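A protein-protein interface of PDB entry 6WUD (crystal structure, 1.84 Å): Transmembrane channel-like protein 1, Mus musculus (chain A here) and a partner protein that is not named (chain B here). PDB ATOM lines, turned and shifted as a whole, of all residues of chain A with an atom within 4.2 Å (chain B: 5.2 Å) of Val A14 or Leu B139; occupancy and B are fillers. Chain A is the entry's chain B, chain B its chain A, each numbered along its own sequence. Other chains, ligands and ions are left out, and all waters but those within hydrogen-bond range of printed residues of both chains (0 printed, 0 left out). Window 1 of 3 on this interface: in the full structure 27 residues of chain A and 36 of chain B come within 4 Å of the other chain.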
ATOM      1  N   PHE A  10      31.747  -7.272  25.052  1.00  0.00           N
ATOM      2  CA  PHE A  10      31.511  -5.830  25.004  1.00  0.00           C
ATOM      3  C   PHE A  10      31.902  -5.243  23.650  1.00  0.00           C
ATOM      4  O   PHE A  10      31.240  -4.320  23.139  1.00  0.00           O
ATOM      5  CB  PHE A  10      32.288  -5.151  26.122  1.00  0.00           C
ATOM      6  CG  PHE A  10      31.704  -5.375  27.498  1.00  0.00           C
ATOM      7  CD1 PHE A  10      31.946  -6.555  28.201  1.00  0.00           C
ATOM      8  CD2 PHE A  10      30.919  -4.399  28.085  1.00  0.00           C
ATOM      9  CE1 PHE A  10      31.413  -6.749  29.465  1.00  0.00           C
ATOM     10  CE2 PHE A  10      30.402  -4.578  29.371  1.00  0.00           C
ATOM     11  CZ  PHE A  10      30.636  -5.759  30.048  1.00  0.00           C
ATOM     12  N   SER A  11      32.953  -5.771  23.020  1.00  0.00           N
ATOM     13  CA  SER A  11      33.356  -5.238  21.713  1.00  0.00           C
ATOM     14  C   SER A  11      32.216  -5.281  20.689  1.00  0.00           C
ATOM     15  O   SER A  11      31.968  -4.297  19.965  1.00  0.00           O
ATOM     16  CB  SER A  11      34.570  -6.004  21.186  1.00  0.00           C
ATOM     17  OG  SER A  11      35.737  -5.581  21.870  1.00  0.00           O
ATOM     18  N   TRP A  12      31.519  -6.415  20.602  1.00  0.00           N
ATOM     19  CA  TRP A  12      30.424  -6.519  19.650  1.00  0.00           C
ATOM     20  C   TRP A  12      29.235  -5.663  20.071  1.00  0.00           C
ATOM     21  O   TRP A  12      28.467  -5.210  19.211  1.00  0.00           O
ATOM     22  CB  TRP A  12      30.028  -7.978  19.476  1.00  0.00           C
ATOM     23  CG  TRP A  12      31.113  -8.770  18.772  1.00  0.00           C
ATOM     24  CD1 TRP A  12      32.254  -8.265  18.199  1.00  0.00           C
ATOM     25  CD2 TRP A  12      31.163 -10.191  18.571  1.00  0.00           C
ATOM     26  NE1 TRP A  12      33.002  -9.279  17.660  1.00  0.00           N
ATOM     27  CE2 TRP A  12      32.351 -10.472  17.861  1.00  0.00           C
ATOM     28  CE3 TRP A  12      30.315 -11.257  18.917  1.00  0.00           C
ATOM     29  CZ2 TRP A  12      32.714 -11.769  17.499  1.00  0.00           C
ATOM     30  CZ3 TRP A  12      30.681 -12.542  18.562  1.00  0.00           C
ATOM     31  CH2 TRP A  12      31.870 -12.791  17.861  1.00  0.00           C
ATOM     32  N   LYS A  13      29.068  -5.408  21.376  1.00  0.00           N
ATOM     33  CA  LYS A  13      28.034  -4.457  21.812  1.00  0.00           C
ATOM     34  C   LYS A  13      28.345  -3.027  21.371  1.00  0.00           C
ATOM     35  O   LYS A  13      27.426  -2.252  21.075  1.00  0.00           O
ATOM     36  CB  LYS A  13      27.855  -4.497  23.336  1.00  0.00           C
ATOM     37  CG  LYS A  13      27.126  -5.744  23.851  1.00  0.00           C
ATOM     38  CD  LYS A  13      27.216  -5.878  25.361  1.00  0.00           C
ATOM     39  CE  LYS A  13      26.544  -7.156  25.877  1.00  0.00           C
ATOM     40  NZ  LYS A  13      26.170  -8.125  24.815  1.00  0.00           N
ATOM     41  N   VAL A  14      29.614  -2.642  21.356  1.00  0.00           N
ATOM     42  CA  VAL A  14      29.979  -1.275  20.989  1.00  0.00           C
ATOM     43  C   VAL A  14      29.965  -1.092  19.477  1.00  0.00           C
ATOM     44  O   VAL A  14      29.565  -0.034  18.986  1.00  0.00           O
ATOM     45  CB  VAL A  14      31.357  -0.921  21.588  1.00  0.00           C
ATOM     46  CG1 VAL A  14      31.857   0.432  21.072  1.00  0.00           C
ATOM     47  CG2 VAL A  14      31.270  -0.911  23.102  1.00  0.00           C
ATOM     48  N   PHE A  15      30.379  -2.106  18.707  1.00  0.00           N
ATOM     49  CA  PHE A  15      30.549  -1.929  17.274  1.00  0.00           C
ATOM     50  C   PHE A  15      29.535  -2.637  16.389  1.00  0.00           C
ATOM     51  O   PHE A  15      29.559  -2.413  15.178  1.00  0.00           O
ATOM     52  CB  PHE A  15      31.963  -2.370  16.881  1.00  0.00           C
ATOM     53  CG  PHE A  15      33.040  -1.554  17.524  1.00  0.00           C
ATOM     54  CD1 PHE A  15      33.169  -0.203  17.206  1.00  0.00           C
ATOM     55  CD2 PHE A  15      33.945  -2.124  18.393  1.00  0.00           C
ATOM     56  CE1 PHE A  15      34.148   0.566  17.774  1.00  0.00           C
ATOM     57  CE2 PHE A  15      34.954  -1.357  18.959  1.00  0.00           C
ATOM     58  CZ  PHE A  15      35.056  -0.010  18.653  1.00  0.00           C
ATOM     59  N   CYS A  16      28.630  -3.435  16.942  1.00  0.00           N
ATOM     60  CA  CYS A  16      27.605  -4.091  16.132  1.00  0.00           C
ATOM     61  C   CYS A  16      26.203  -3.914  16.702  1.00  0.00           C
ATOM     62  O   CYS A  16      25.358  -4.793  16.536  1.00  0.00           O
ATOM     63  CB  CYS A  16      27.883  -5.584  15.986  1.00  0.00           C
ATOM     64  SG  CYS A  16      29.545  -6.004  15.473  1.00  0.00           S
ATOM     65  N   TRP A  18      24.235  -0.538  16.714  1.00  0.00           N
ATOM     66  CA  TRP A  18      23.322   0.338  16.009  1.00  0.00           C
ATOM     67  C   TRP A  18      22.908  -0.252  14.664  1.00  0.00           C
ATOM     68  O   TRP A  18      23.757  -0.626  13.878  1.00  0.00           O
ATOM     69  CB  TRP A  18      23.888   1.738  15.795  1.00  0.00           C
ATOM     70  CG  TRP A  18      22.820   2.604  15.264  1.00  0.00           C
ATOM     71  CD1 TRP A  18      22.672   3.035  13.988  1.00  0.00           C
ATOM     72  CD2 TRP A  18      21.670   3.054  15.976  1.00  0.00           C
ATOM     73  NE1 TRP A  18      21.520   3.761  13.865  1.00  0.00           N
ATOM     74  CE2 TRP A  18      20.888   3.791  15.078  1.00  0.00           C
ATOM     75  CE3 TRP A  18      21.243   2.929  17.297  1.00  0.00           C
ATOM     76  CZ2 TRP A  18      19.702   4.398  15.457  1.00  0.00           C
ATOM     77  CZ3 TRP A  18      20.072   3.526  17.666  1.00  0.00           C
ATOM     78  CH2 TRP A  18      19.314   4.254  16.753  1.00  0.00           C
ATOM     79  N   PHE A  32      17.816   2.745  21.007  1.00  0.00           N
ATOM     80  CA  PHE A  32      18.654   3.334  22.036  1.00  0.00           C
ATOM     81  C   PHE A  32      18.324   2.755  23.416  1.00  0.00           C
ATOM     82  O   PHE A  32      19.228   2.458  24.208  1.00  0.00           O
ATOM     83  CB  PHE A  32      18.463   4.857  22.081  1.00  0.00           C
ATOM     84  CG  PHE A  32      19.186   5.603  20.991  1.00  0.00           C
ATOM     85  CD1 PHE A  32      20.586   5.584  20.908  1.00  0.00           C
ATOM     86  CD2 PHE A  32      18.460   6.360  20.050  1.00  0.00           C
ATOM     87  CE1 PHE A  32      21.234   6.258  19.889  1.00  0.00           C
ATOM     88  CE2 PHE A  32      19.122   7.029  19.027  1.00  0.00           C
ATOM     89  CZ  PHE A  32      20.511   6.988  18.974  1.00  0.00           C
ATOM     90  N   ILE A  35      19.614  -0.906  23.560  1.00  0.00           N
ATOM     91  CA  ILE A  35      21.071  -0.953  23.658  1.00  0.00           C
ATOM     92  C   ILE A  35      21.522  -0.562  25.059  1.00  0.00           C
ATOM     93  O   ILE A  35      22.386  -1.213  25.667  1.00  0.00           O
ATOM     94  CB  ILE A  35      21.689  -0.026  22.595  1.00  0.00           C
ATOM     95  CG1 ILE A  35      21.443  -0.571  21.186  1.00  0.00           C
ATOM     96  CG2 ILE A  35      23.218   0.151  22.849  1.00  0.00           C
ATOM     97  CD1 ILE A  35      21.882   0.385  20.065  1.00  0.00           C
ATOM     98  N   PHE A  39      23.597  -2.835  27.749  1.00  0.00           N
ATOM     99  CA  PHE A  39      24.865  -2.496  28.401  1.00  0.00           C
ATOM    100  C   PHE A  39      24.753  -2.613  29.924  1.00  0.00           C
ATOM    101  O   PHE A  39      25.674  -3.094  30.601  1.00  0.00           O
ATOM    102  CB  PHE A  39      25.312  -1.077  28.016  1.00  0.00           C
ATOM    103  CG  PHE A  39      26.113  -1.002  26.736  1.00  0.00           C
ATOM    104  CD1 PHE A  39      27.362  -1.592  26.642  1.00  0.00           C
ATOM    105  CD2 PHE A  39      25.611  -0.337  25.641  1.00  0.00           C
ATOM    106  CE1 PHE A  39      28.095  -1.523  25.460  1.00  0.00           C
ATOM    107  CE2 PHE A  39      26.324  -0.264  24.455  1.00  0.00           C
ATOM    108  CZ  PHE A  39      27.587  -0.849  24.365  1.00  0.00           C
ATOM    109  N   PRO B  73      23.000   7.786  15.140  1.00  0.00           N
ATOM    110  CA  PRO B  73      23.831   8.619  16.038  1.00  0.00           C
ATOM    111  C   PRO B  73      25.214   8.940  15.459  1.00  0.00           C
ATOM    112  O   PRO B  73      25.840   9.917  15.902  1.00  0.00           O
ATOM    113  CB  PRO B  73      23.926   7.784  17.322  1.00  0.00           C
ATOM    114  CG  PRO B  73      23.769   6.321  16.856  1.00  0.00           C
ATOM    115  CD  PRO B  73      22.787   6.422  15.672  1.00  0.00           C
ATOM    116  N   PHE B  74      25.682   8.185  14.471  1.00  0.00           N
ATOM    117  CA  PHE B  74      26.990   8.364  13.845  1.00  0.00           C
ATOM    118  C   PHE B  74      26.925   9.095  12.510  1.00  0.00           C
ATOM    119  O   PHE B  74      27.944   9.176  11.804  1.00  0.00           O
ATOM    120  CB  PHE B  74      27.642   6.995  13.691  1.00  0.00           C
ATOM    121  CG  PHE B  74      27.761   6.263  14.977  1.00  0.00           C
ATOM    122  CD1 PHE B  74      27.081   5.064  15.179  1.00  0.00           C
ATOM    123  CD2 PHE B  74      28.503   6.796  16.021  1.00  0.00           C
ATOM    124  CE1 PHE B  74      27.176   4.409  16.402  1.00  0.00           C
ATOM    125  CE2 PHE B  74      28.614   6.119  17.239  1.00  0.00           C
ATOM    126  CZ  PHE B  74      27.932   4.922  17.422  1.00  0.00           C
ATOM    127  N   LEU B 132      36.568   5.433  22.086  1.00  0.00           N
ATOM    128  CA  LEU B 132      35.556   4.495  22.562  1.00  0.00           C
ATOM    129  C   LEU B 132      34.511   5.208  23.422  1.00  0.00           C
ATOM    130  O   LEU B 132      33.307   4.887  23.376  1.00  0.00           O
ATOM    131  CB  LEU B 132      36.239   3.378  23.353  1.00  0.00           C
ATOM    132  CG  LEU B 132      36.957   2.282  22.569  1.00  0.00           C
ATOM    133  CD1 LEU B 132      37.712   1.378  23.566  1.00  0.00           C
ATOM    134  CD2 LEU B 132      36.030   1.471  21.717  1.00  0.00           C
ATOM    135  N   GLN B 134      33.512   8.283  23.036  1.00  0.00           N
ATOM    136  CA  GLN B 134      32.596   8.977  22.127  1.00  0.00           C
ATOM    137  C   GLN B 134      31.582   8.007  21.540  1.00  0.00           C
ATOM    138  O   GLN B 134      30.382   8.295  21.490  1.00  0.00           O
ATOM    139  CB  GLN B 134      33.355   9.669  20.993  1.00  0.00           C
ATOM    140  CG  GLN B 134      34.503  10.597  21.436  1.00  0.00           C
ATOM    141  CD  GLN B 134      34.172  11.453  22.625  1.00  0.00           C
ATOM    142  OE1 GLN B 134      33.350  12.360  22.525  1.00  0.00           O
ATOM    143  NE2 GLN B 134      34.818  11.181  23.768  1.00  0.00           N
ATOM    144  N   THR B 135      32.059   6.846  21.083  1.00  0.00           N
ATOM    145  CA  THR B 135      31.179   5.839  20.501  1.00  0.00           C
ATOM    146  C   THR B 135      30.118   5.366  21.493  1.00  0.00           C
ATOM    147  O   THR B 135      28.916   5.374  21.186  1.00  0.00           O
ATOM    148  CB  THR B 135      32.017   4.665  19.985  1.00  0.00           C
ATOM    149  OG1 THR B 135      32.998   5.144  19.038  1.00  0.00           O
ATOM    150  CG2 THR B 135      31.100   3.647  19.313  1.00  0.00           C
ATOM    151  N   VAL B 136      30.539   4.976  22.701  1.00  0.00           N
ATOM    152  CA  VAL B 136      29.585   4.471  23.681  1.00  0.00           C
ATOM    153  C   VAL B 136      28.587   5.546  24.066  1.00  0.00           C
ATOM    154  O   VAL B 136      27.391   5.265  24.258  1.00  0.00           O
ATOM    155  CB  VAL B 136      30.328   3.919  24.916  1.00  0.00           C
ATOM    156  CG1 VAL B 136      29.358   3.592  26.001  1.00  0.00           C
ATOM    157  CG2 VAL B 136      31.115   2.667  24.528  1.00  0.00           C
ATOM    158  N   THR B 137      29.060   6.789  24.211  1.00  0.00           N
ATOM    159  CA  THR B 137      28.181   7.884  24.589  1.00  0.00           C
ATOM    160  C   THR B 137      27.082   8.093  23.553  1.00  0.00           C
ATOM    161  O   THR B 137      25.901   8.249  23.893  1.00  0.00           O
ATOM    162  CB  THR B 137      29.001   9.160  24.768  1.00  0.00           C
ATOM    163  OG1 THR B 137      29.894   9.016  25.894  1.00  0.00           O
ATOM    164  CG2 THR B 137      28.082  10.352  25.019  1.00  0.00           C
ATOM    165  N   LYS B 138      27.456   8.149  22.282  1.00  0.00           N
ATOM    166  CA  LYS B 138      26.453   8.303  21.233  1.00  0.00           C
ATOM    167  C   LYS B 138      25.498   7.116  21.159  1.00  0.00           C
ATOM    168  O   LYS B 138      24.296   7.301  20.901  1.00  0.00           O
ATOM    169  CB  LYS B 138      27.162   8.520  19.898  1.00  0.00           C
ATOM    170  CG  LYS B 138      28.001   9.776  19.903  1.00  0.00           C
ATOM    171  CD  LYS B 138      28.499  10.123  18.524  1.00  0.00           C
ATOM    172  CE  LYS B 138      28.201  11.581  18.204  1.00  0.00           C
ATOM    173  NZ  LYS B 138      29.147  12.481  18.913  1.00  0.00           N
ATOM    174  N   LEU B 139      25.993   5.908  21.427  1.00  0.00           N
ATOM    175  CA  LEU B 139      25.152   4.730  21.334  1.00  0.00           C
ATOM    176  C   LEU B 139      24.093   4.688  22.404  1.00  0.00           C
ATOM    177  O   LEU B 139      23.066   4.019  22.208  1.00  0.00           O
ATOM    178  CB  LEU B 139      25.998   3.478  21.468  1.00  0.00           C
ATOM    179  CG  LEU B 139      26.507   2.703  20.273  1.00  0.00           C
ATOM    180  CD1 LEU B 139      27.210   1.512  20.909  1.00  0.00           C
ATOM    181  CD2 LEU B 139      25.395   2.348  19.336  1.00  0.00           C
ATOM    182  N   THR B 140      24.319   5.390  23.521  1.00  0.00           N
ATOM    183  CA  THR B 140      23.436   5.383  24.671  1.00  0.00           C
ATOM    184  C   THR B 140      22.925   6.779  24.986  1.00  0.00           C
ATOM    185  O   THR B 140      22.267   6.972  26.015  1.00  0.00           O
ATOM    186  CB  THR B 140      24.179   4.798  25.871  1.00  0.00           C
ATOM    187  OG1 THR B 140      25.318   5.623  26.158  1.00  0.00           O
ATOM    188  CG2 THR B 140      24.659   3.373  25.568  1.00  0.00           C
ATOM    189  N   ARG B 141      23.143   7.739  24.086  1.00  0.00           N
ATOM    190  CA  ARG B 141      22.642   9.104  24.260  1.00  0.00           C
ATOM    191  C   ARG B 141      22.955   9.638  25.653  1.00  0.00           C
ATOM    192  O   ARG B 141      22.127  10.285  26.297  1.00  0.00           O
ATOM    193  CB  ARG B 141      21.135   9.198  23.998  1.00  0.00           C
ATOM    194  CG  ARG B 141      20.684   8.588  22.710  1.00  0.00           C
ATOM    195  CD  ARG B 141      19.200   8.862  22.525  1.00  0.00           C
ATOM    196  NE  ARG B 141      18.401   7.938  23.322  1.00  0.00           N
ATOM    197  CZ  ARG B 141      17.086   7.782  23.199  1.00  0.00           C
ATOM    198  NH1 ARG B 141      16.386   8.511  22.317  1.00  0.00           N
ATOM    199  NH2 ARG B 141      16.463   6.900  23.975  1.00  0.00           N
ATOM    200  N   VAL B 152      33.010  -0.128  30.214  1.00  0.00           N
ATOM    201  CA  VAL B 152      32.822  -0.665  28.869  1.00  0.00           C
ATOM    202  C   VAL B 152      34.078  -0.448  28.034  1.00  0.00           C
ATOM    203  O   VAL B 152      34.566  -1.353  27.345  1.00  0.00           O
ATOM    204  CB  VAL B 152      31.599  -0.021  28.191  1.00  0.00           C
ATOM    205  CG1 VAL B 152      31.488  -0.530  26.721  1.00  0.00           C
ATOM    206  CG2 VAL B 152      30.339  -0.297  28.966  1.00  0.00           C
ATOM    207  N   VAL B 156      36.412  -3.358  26.270  1.00  0.00           N
ATOM    208  CA  VAL B 156      36.667  -3.475  24.855  1.00  0.00           C
ATOM    209  C   VAL B 156      38.169  -3.539  24.602  1.00  0.00           C
ATOM    210  O   VAL B 156      38.616  -4.373  23.869  1.00  0.00           O
ATOM    211  CB  VAL B 156      36.081  -2.286  24.092  1.00  0.00           C
ATOM    212  CG1 VAL B 156      36.491  -2.366  22.649  1.00  0.00           C
ATOM    213  CG2 VAL B 156      34.570  -2.269  24.222  1.00  0.00           C
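Of the 11 printed residues of chain A, 8 touch a printed residue of chain B.
Printed residues of chain A that touch a printed residue of chain B: Ser A11, Lys A13, Val A14, Phe A15, Trp A18, Phe A32, Ile A35 and Phe A39.
Among the printed residues, no Asp or Glu carboxylate lies within 4 Å of a Lys or Arg side-chain nitrogen of the other chain.
Lys A13 touches Leu B139.
Val A14 touches Thr B135 (CG1 to CG2, 3.7 Å).
Val A14 touches Leu B139.
Val A14 touches Val B152 (CG2 to CG1, 3.6 Å).
Val A14 touches Val B156.
Trp A18 touches Pro B73.
Trp A18 touches Leu B139 (CB to CD2, 3.9 Å).
Phe A32 touches Arg B141 (CB to NE, 3.3 Å).
Ile A35 touches Leu B139.
Thr B140 touches Phe A39 (CG2 to CD2, 3.8 Å).
Val A14 touches five residues of chain B.
Of the printed residues of chain B, Phe A15 touches Leu B132 (3.5 Å).
Cys A16 touches none of the printed residues of chain B.
Of the printed residues of chain A, Pro B73 touches Trp A18 (3.3 Å) and Phe A32 (3.9 Å).
Phe B74 touches none of the printed residues of chain A.
Printed residues of chain A within 4 Å of Thr B135: Val A14 (3.7 Å).
Of chain A, only Lys A13 (3.8 Å), Val A14 (3.4 Å), Trp A18 (3.9 Å), Phe A32 (3.2 Å) and Ile A35 (3.9 Å) come within 4 Å of Leu B139.
Of the printed residues of chain A, Thr B140 touches Phe A39 (3.8 Å).
The nearest residue of chain B that does not touch Val A14 is Leu B132 (4.3 Å).
The nearest residue of chain A that does not touch Leu B139 is Phe A39 (4.1 Å).
The nearest printed residue of chain B that does not touch Trp A18 is Phe B74 (4.3 Å).
O of Val B136 is in hydrogen-bond range of OG1 of Thr B140 (2.8 Å).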
